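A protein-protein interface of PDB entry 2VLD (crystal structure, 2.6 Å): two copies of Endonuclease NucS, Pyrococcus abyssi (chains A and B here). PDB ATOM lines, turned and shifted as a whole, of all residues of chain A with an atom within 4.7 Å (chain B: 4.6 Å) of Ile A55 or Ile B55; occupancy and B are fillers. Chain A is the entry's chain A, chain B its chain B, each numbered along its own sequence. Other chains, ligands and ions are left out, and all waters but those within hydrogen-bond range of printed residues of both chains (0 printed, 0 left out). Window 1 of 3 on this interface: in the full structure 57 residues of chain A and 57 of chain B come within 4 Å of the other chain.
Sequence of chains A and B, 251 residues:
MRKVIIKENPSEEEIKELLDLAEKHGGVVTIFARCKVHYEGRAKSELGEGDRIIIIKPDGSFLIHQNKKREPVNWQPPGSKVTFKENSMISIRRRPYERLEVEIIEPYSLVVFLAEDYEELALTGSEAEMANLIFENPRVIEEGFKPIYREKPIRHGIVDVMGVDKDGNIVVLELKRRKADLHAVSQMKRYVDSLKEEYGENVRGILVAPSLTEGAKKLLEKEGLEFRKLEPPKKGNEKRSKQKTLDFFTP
O of Leu B63 is in hydrogen-bond range of N of Ile B55 (2.8 Å).
The backbone NH (N) of Ile A55 sits at hydrogen-bond distance from the backbone carbonyl oxygen (O) of Leu A63, at 2.9 Å.
CD1 of Ile B53 touches CG1 of Val A28, at 3.6 Å.
Thr A30 touches Ile B53 (OG1 to CD1, 3.8 Å).
Ile A53 touches Val B28.
Ile A53 touches Thr B30.
Ile B55 touches Ile A55.
Ile A55 touches just one residue of chain B: Ile B55 (3.6 Å).
Printed residues of chain B within 4 Å of Thr A30: Ile B53 (3.8 Å).
Of the printed residues of chain B, Val A28 touches Ile B53 (3.6 Å).
Printed residues of chain A within 4 Å of Thr B30: Ile A53.
Val A28 touches Ile B53, and with the chains exchanged Ile A53 touches Val B28.
Thr A30 touches Ile B53, and with the chains exchanged Ile A53 touches Thr B30.
Ile A55 touches its own counterpart, Ile B55.
11 positions are printed for both chains.
Of the 5 pairs that touch across the chains among the printed residues, 5 have their exchanged pair printed and touching as well.
Of the 11 printed residues of chain B, 4 touch a printed residue of chain A.
Hydrophobic or aromatic side chains of chain B within 4 Å of the printed part of chain A: Val B28, Ile B53 and Ile B55.
Of the 11 printed residues of chain A, 4 touch a printed residue of chain B.
Hydrophobic or aromatic side chains of chain A that line the printed part of chain B: Val A28, Ile A53 and Ile A55.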
ATOM      1  N   VAL A  28       9.899 -25.894 -22.841  1.00  0.00           N
ATOM      2  CA  VAL A  28      11.021 -25.600 -21.948  1.00  0.00           C
ATOM      3  C   VAL A  28      11.738 -26.907 -21.636  1.00  0.00           C
ATOM      4  O   VAL A  28      11.093 -27.896 -21.248  1.00  0.00           O
ATOM      5  CB  VAL A  28      10.561 -24.922 -20.629  1.00  0.00           C
ATOM      6  CG1 VAL A  28      11.742 -24.680 -19.684  1.00  0.00           C
ATOM      7  CG2 VAL A  28       9.847 -23.619 -20.917  1.00  0.00           C
ATOM      8  N   VAL A  29      13.064 -26.908 -21.825  1.00  0.00           N
ATOM      9  CA  VAL A  29      13.921 -28.036 -21.433  1.00  0.00           C
ATOM     10  C   VAL A  29      14.487 -27.801 -20.037  1.00  0.00           C
ATOM     11  O   VAL A  29      15.039 -26.734 -19.766  1.00  0.00           O
ATOM     12  CB  VAL A  29      15.100 -28.240 -22.413  1.00  0.00           C
ATOM     13  CG1 VAL A  29      15.792 -29.581 -22.168  1.00  0.00           C
ATOM     14  CG2 VAL A  29      14.625 -28.151 -23.860  1.00  0.00           C
ATOM     15  N   THR A  30      14.336 -28.787 -19.155  1.00  0.00           N
ATOM     16  CA  THR A  30      14.975 -28.753 -17.841  1.00  0.00           C
ATOM     17  C   THR A  30      15.781 -30.033 -17.649  1.00  0.00           C
ATOM     18  O   THR A  30      15.215 -31.131 -17.592  1.00  0.00           O
ATOM     19  CB  THR A  30      13.961 -28.611 -16.696  1.00  0.00           C
ATOM     20  OG1 THR A  30      13.152 -27.456 -16.910  1.00  0.00           O
ATOM     21  CG2 THR A  30      14.672 -28.467 -15.350  1.00  0.00           C
ATOM     22  N   ILE A  53      20.971 -27.839 -12.274  1.00  0.00           N
ATOM     23  CA  ILE A  53      19.715 -27.829 -13.010  1.00  0.00           C
ATOM     24  C   ILE A  53      19.853 -26.787 -14.109  1.00  0.00           C
ATOM     25  O   ILE A  53      20.266 -25.655 -13.836  1.00  0.00           O
ATOM     26  CB  ILE A  53      18.528 -27.428 -12.122  1.00  0.00           C
ATOM     27  CG1 ILE A  53      18.470 -28.318 -10.879  1.00  0.00           C
ATOM     28  CG2 ILE A  53      17.245 -27.545 -12.900  1.00  0.00           C
ATOM     29  CD1 ILE A  53      17.339 -27.991  -9.931  1.00  0.00           C
ATOM     30  N   ILE A  54      19.509 -27.168 -15.332  1.00  0.00           N
ATOM     31  CA  ILE A  54      19.750 -26.337 -16.494  1.00  0.00           C
ATOM     32  C   ILE A  54      18.424 -26.118 -17.215  1.00  0.00           C
ATOM     33  O   ILE A  54      17.757 -27.097 -17.604  1.00  0.00           O
ATOM     34  CB  ILE A  54      20.751 -27.020 -17.467  1.00  0.00           C
ATOM     35  CG1 ILE A  54      22.144 -27.131 -16.844  1.00  0.00           C
ATOM     36  CG2 ILE A  54      20.848 -26.252 -18.775  1.00  0.00           C
ATOM     37  CD1 ILE A  54      22.464 -28.485 -16.292  1.00  0.00           C
ATOM     38  N   ILE A  55      18.058 -24.851 -17.420  1.00  0.00           N
ATOM     39  CA  ILE A  55      16.760 -24.492 -17.975  1.00  0.00           C
ATOM     40  C   ILE A  55      16.946 -23.773 -19.311  1.00  0.00           C
ATOM     41  O   ILE A  55      17.668 -22.783 -19.398  1.00  0.00           O
ATOM     42  CB  ILE A  55      15.948 -23.641 -16.964  1.00  0.00           C
ATOM     43  CG1 ILE A  55      15.645 -24.469 -15.714  1.00  0.00           C
ATOM     44  CG2 ILE A  55      14.648 -23.160 -17.567  1.00  0.00           C
ATOM     45  CD1 ILE A  55      15.051 -23.692 -14.553  1.00  0.00           C
ATOM     46  N   ILE A  56      16.315 -24.293 -20.354  1.00  0.00           N
ATOM     47  CA  ILE A  56      16.447 -23.723 -21.674  1.00  0.00           C
ATOM     48  C   ILE A  56      15.047 -23.347 -22.123  1.00  0.00           C
ATOM     49  O   ILE A  56      14.163 -24.201 -22.250  1.00  0.00           O
ATOM     50  CB  ILE A  56      17.081 -24.725 -22.684  1.00  0.00           C
ATOM     51  CG1 ILE A  56      18.388 -25.312 -22.128  1.00  0.00           C
ATOM     52  CG2 ILE A  56      17.297 -24.062 -24.037  1.00  0.00           C
ATOM     53  CD1 ILE A  56      18.907 -26.528 -22.899  1.00  0.00           C
ATOM     54  N   LYS A  57      14.839 -22.060 -22.343  1.00  0.00           N
ATOM     55  CA  LYS A  57      13.533 -21.569 -22.729  1.00  0.00           C
ATOM     56  C   LYS A  57      13.491 -21.328 -24.218  1.00  0.00           C
ATOM     57  O   LYS A  57      14.527 -21.053 -24.830  1.00  0.00           O
ATOM     58  CB  LYS A  57      13.221 -20.278 -21.992  1.00  0.00           C
ATOM     59  CG  LYS A  57      13.253 -20.433 -20.510  1.00  0.00           C
ATOM     60  CD  LYS A  57      12.589 -19.284 -19.826  1.00  0.00           C
ATOM     61  CE  LYS A  57      12.629 -19.519 -18.323  1.00  0.00           C
ATOM     62  NZ  LYS A  57      12.206 -18.295 -17.580  1.00  0.00           N
ATOM     63  N   SER A  61      16.519 -18.098 -23.500  1.00  0.00           N
ATOM     64  CA  SER A  61      16.928 -17.963 -22.104  1.00  0.00           C
ATOM     65  C   SER A  61      17.556 -19.266 -21.628  1.00  0.00           C
ATOM     66  O   SER A  61      16.983 -20.334 -21.813  1.00  0.00           O
ATOM     67  CB  SER A  61      15.715 -17.641 -21.236  1.00  0.00           C
ATOM     68  OG  SER A  61      15.141 -16.393 -21.573  1.00  0.00           O
ATOM     69  N   PHE A  62      18.721 -19.178 -21.002  1.00  0.00           N
ATOM     70  CA  PHE A  62      19.467 -20.357 -20.599  1.00  0.00           C
ATOM     71  C   PHE A  62      19.939 -20.091 -19.174  1.00  0.00           C
ATOM     72  O   PHE A  62      20.525 -19.032 -18.934  1.00  0.00           O
ATOM     73  CB  PHE A  62      20.670 -20.500 -21.532  1.00  0.00           C
ATOM     74  CG  PHE A  62      21.365 -21.816 -21.433  1.00  0.00           C
ATOM     75  CD1 PHE A  62      22.329 -22.045 -20.455  1.00  0.00           C
ATOM     76  CD2 PHE A  62      21.090 -22.824 -22.344  1.00  0.00           C
ATOM     77  CE1 PHE A  62      22.991 -23.287 -20.371  1.00  0.00           C
ATOM     78  CE2 PHE A  62      21.739 -24.063 -22.271  1.00  0.00           C
ATOM     79  CZ  PHE A  62      22.688 -24.294 -21.279  1.00  0.00           C
ATOM     80  N   LEU A  63      19.664 -21.001 -18.236  1.00  0.00           N
ATOM     81  CA  LEU A  63      19.957 -20.761 -16.841  1.00  0.00           C
ATOM     82  C   LEU A  63      20.585 -21.990 -16.233  1.00  0.00           C
ATOM     83  O   LEU A  63      20.141 -23.114 -16.500  1.00  0.00           O
ATOM     84  CB  LEU A  63      18.677 -20.456 -16.031  1.00  0.00           C
ATOM     85  CG  LEU A  63      17.668 -19.501 -16.660  1.00  0.00           C
ATOM     86  CD1 LEU A  63      16.383 -19.532 -15.882  1.00  0.00           C
ATOM     87  CD2 LEU A  63      18.273 -18.153 -16.611  1.00  0.00           C
ATOM     88  N   VAL B  28      16.635 -30.717  -4.060  1.00  0.00           N
ATOM     89  CA  VAL B  28      15.936 -29.640  -4.747  1.00  0.00           C
ATOM     90  C   VAL B  28      14.619 -30.181  -5.300  1.00  0.00           C
ATOM     91  O   VAL B  28      14.600 -31.241  -5.928  1.00  0.00           O
ATOM     92  CB  VAL B  28      16.789 -29.028  -5.877  1.00  0.00           C
ATOM     93  CG1 VAL B  28      16.036 -27.871  -6.563  1.00  0.00           C
ATOM     94  CG2 VAL B  28      18.135 -28.545  -5.331  1.00  0.00           C
ATOM     95  N   VAL B  29      13.526 -29.458  -5.030  1.00  0.00           N
ATOM     96  CA  VAL B  29      12.208 -29.746  -5.594  1.00  0.00           C
ATOM     97  C   VAL B  29      12.004 -28.868  -6.819  1.00  0.00           C
ATOM     98  O   VAL B  29      12.188 -27.653  -6.747  1.00  0.00           O
ATOM     99  CB  VAL B  29      11.079 -29.411  -4.589  1.00  0.00           C
ATOM    100  CG1 VAL B  29       9.706 -29.915  -5.093  1.00  0.00           C
ATOM    101  CG2 VAL B  29      11.398 -29.987  -3.213  1.00  0.00           C
ATOM    102  N   THR B  30      11.633 -29.484  -7.939  1.00  0.00           N
ATOM    103  CA  THR B  30      11.228 -28.751  -9.137  1.00  0.00           C
ATOM    104  C   THR B  30       9.827 -29.196  -9.563  1.00  0.00           C
ATOM    105  O   THR B  30       9.629 -30.353  -9.939  1.00  0.00           O
ATOM    106  CB  THR B  30      12.213 -28.947 -10.296  1.00  0.00           C
ATOM    107  OG1 THR B  30      13.508 -28.499  -9.895  1.00  0.00           O
ATOM    108  CG2 THR B  30      11.777 -28.135 -11.503  1.00  0.00           C
ATOM    109  N   ILE B  53       7.370 -23.166 -13.819  1.00  0.00           N
ATOM    110  CA  ILE B  53       8.321 -24.065 -13.169  1.00  0.00           C
ATOM    111  C   ILE B  53       8.706 -23.463 -11.829  1.00  0.00           C
ATOM    112  O   ILE B  53       9.066 -22.278 -11.749  1.00  0.00           O
ATOM    113  CB  ILE B  53       9.605 -24.240 -13.997  1.00  0.00           C
ATOM    114  CG1 ILE B  53       9.274 -24.662 -15.427  1.00  0.00           C
ATOM    115  CG2 ILE B  53      10.502 -25.240 -13.347  1.00  0.00           C
ATOM    116  CD1 ILE B  53      10.492 -24.826 -16.315  1.00  0.00           C
ATOM    117  N   ILE B  54       8.637 -24.272 -10.779  1.00  0.00           N
ATOM    118  CA  ILE B  54       8.859 -23.780  -9.432  1.00  0.00           C
ATOM    119  C   ILE B  54      10.016 -24.551  -8.822  1.00  0.00           C
ATOM    120  O   ILE B  54       9.994 -25.784  -8.808  1.00  0.00           O
ATOM    121  CB  ILE B  54       7.588 -23.945  -8.556  1.00  0.00           C
ATOM    122  CG1 ILE B  54       6.456 -23.080  -9.085  1.00  0.00           C
ATOM    123  CG2 ILE B  54       7.861 -23.593  -7.103  1.00  0.00           C
ATOM    124  CD1 ILE B  54       5.472 -23.847  -9.881  1.00  0.00           C
ATOM    125  N   ILE B  55      11.014 -23.830  -8.311  1.00  0.00           N
ATOM    126  CA  ILE B  55      12.229 -24.454  -7.804  1.00  0.00           C
ATOM    127  C   ILE B  55      12.379 -24.125  -6.334  1.00  0.00           C
ATOM    128  O   ILE B  55      12.355 -22.951  -5.946  1.00  0.00           O
ATOM    129  CB  ILE B  55      13.468 -24.005  -8.623  1.00  0.00           C
ATOM    130  CG1 ILE B  55      13.340 -24.489 -10.079  1.00  0.00           C
ATOM    131  CG2 ILE B  55      14.749 -24.532  -8.007  1.00  0.00           C
ATOM    132  CD1 ILE B  55      14.429 -24.029 -10.997  1.00  0.00           C
ATOM    133  N   ILE B  56      12.513 -25.158  -5.507  1.00  0.00           N
ATOM    134  CA  ILE B  56      12.638 -24.974  -4.066  1.00  0.00           C
ATOM    135  C   ILE B  56      13.943 -25.605  -3.626  1.00  0.00           C
ATOM    136  O   ILE B  56      14.129 -26.824  -3.722  1.00  0.00           O
ATOM    137  CB  ILE B  56      11.457 -25.610  -3.295  1.00  0.00           C
ATOM    138  CG1 ILE B  56      10.110 -25.134  -3.869  1.00  0.00           C
ATOM    139  CG2 ILE B  56      11.576 -25.324  -1.789  1.00  0.00           C
ATOM    140  CD1 ILE B  56       8.878 -25.898  -3.358  1.00  0.00           C
ATOM    141  N   LYS B  57      14.857 -24.769  -3.156  1.00  0.00           N
ATOM    142  CA  LYS B  57      16.171 -25.238  -2.762  1.00  0.00           C
ATOM    143  C   LYS B  57      16.252 -25.434  -1.257  1.00  0.00           C
ATOM    144  O   LYS B  57      15.562 -24.751  -0.498  1.00  0.00           O
ATOM    145  CB  LYS B  57      17.225 -24.247  -3.208  1.00  0.00           C
ATOM    146  CG  LYS B  57      17.235 -24.013  -4.681  1.00  0.00           C
ATOM    147  CD  LYS B  57      18.495 -23.340  -5.055  1.00  0.00           C
ATOM    148  CE  LYS B  57      18.478 -23.012  -6.533  1.00  0.00           C
ATOM    149  NZ  LYS B  57      19.666 -22.166  -6.796  1.00  0.00           N
ATOM    150  N   SER B  61      15.709 -21.054  -0.919  1.00  0.00           N
ATOM    151  CA  SER B  61      15.580 -20.315  -2.164  1.00  0.00           C
ATOM    152  C   SER B  61      14.345 -20.815  -2.879  1.00  0.00           C
ATOM    153  O   SER B  61      14.157 -22.030  -3.032  1.00  0.00           O
ATOM    154  CB  SER B  61      16.802 -20.504  -3.045  1.00  0.00           C
ATOM    155  OG  SER B  61      17.948 -19.937  -2.437  1.00  0.00           O
ATOM    156  N   PHE B  62      13.504 -19.882  -3.308  1.00  0.00           N
ATOM    157  CA  PHE B  62      12.257 -20.219  -3.984  1.00  0.00           C
ATOM    158  C   PHE B  62      12.151 -19.419  -5.307  1.00  0.00           C
ATOM    159  O   PHE B  62      12.228 -18.199  -5.285  1.00  0.00           O
ATOM    160  CB  PHE B  62      11.104 -19.875  -3.036  1.00  0.00           C
ATOM    161  CG  PHE B  62       9.789 -20.501  -3.409  1.00  0.00           C
ATOM    162  CD1 PHE B  62       8.970 -19.915  -4.370  1.00  0.00           C
ATOM    163  CD2 PHE B  62       9.349 -21.646  -2.776  1.00  0.00           C
ATOM    164  CE1 PHE B  62       7.736 -20.491  -4.710  1.00  0.00           C
ATOM    165  CE2 PHE B  62       8.119 -22.223  -3.110  1.00  0.00           C
ATOM    166  CZ  PHE B  62       7.317 -21.654  -4.070  1.00  0.00           C
ATOM    167  N   LEU B  63      12.000 -20.091  -6.441  1.00  0.00           N
ATOM    168  CA  LEU B  63      11.965 -19.396  -7.744  1.00  0.00           C
ATOM    169  C   LEU B  63      10.778 -19.849  -8.532  1.00  0.00           C
ATOM    170  O   LEU B  63      10.472 -21.047  -8.554  1.00  0.00           O
ATOM    171  CB  LEU B  63      13.208 -19.693  -8.594  1.00  0.00           C
ATOM    172  CG  LEU B  63      14.541 -19.696  -7.845  1.00  0.00           C
ATOM    173  CD1 LEU B  63      15.683 -20.243  -8.699  1.00  0.00           C
ATOM    174  CD2 LEU B  63      14.817 -18.265  -7.452  1.00  0.00           C
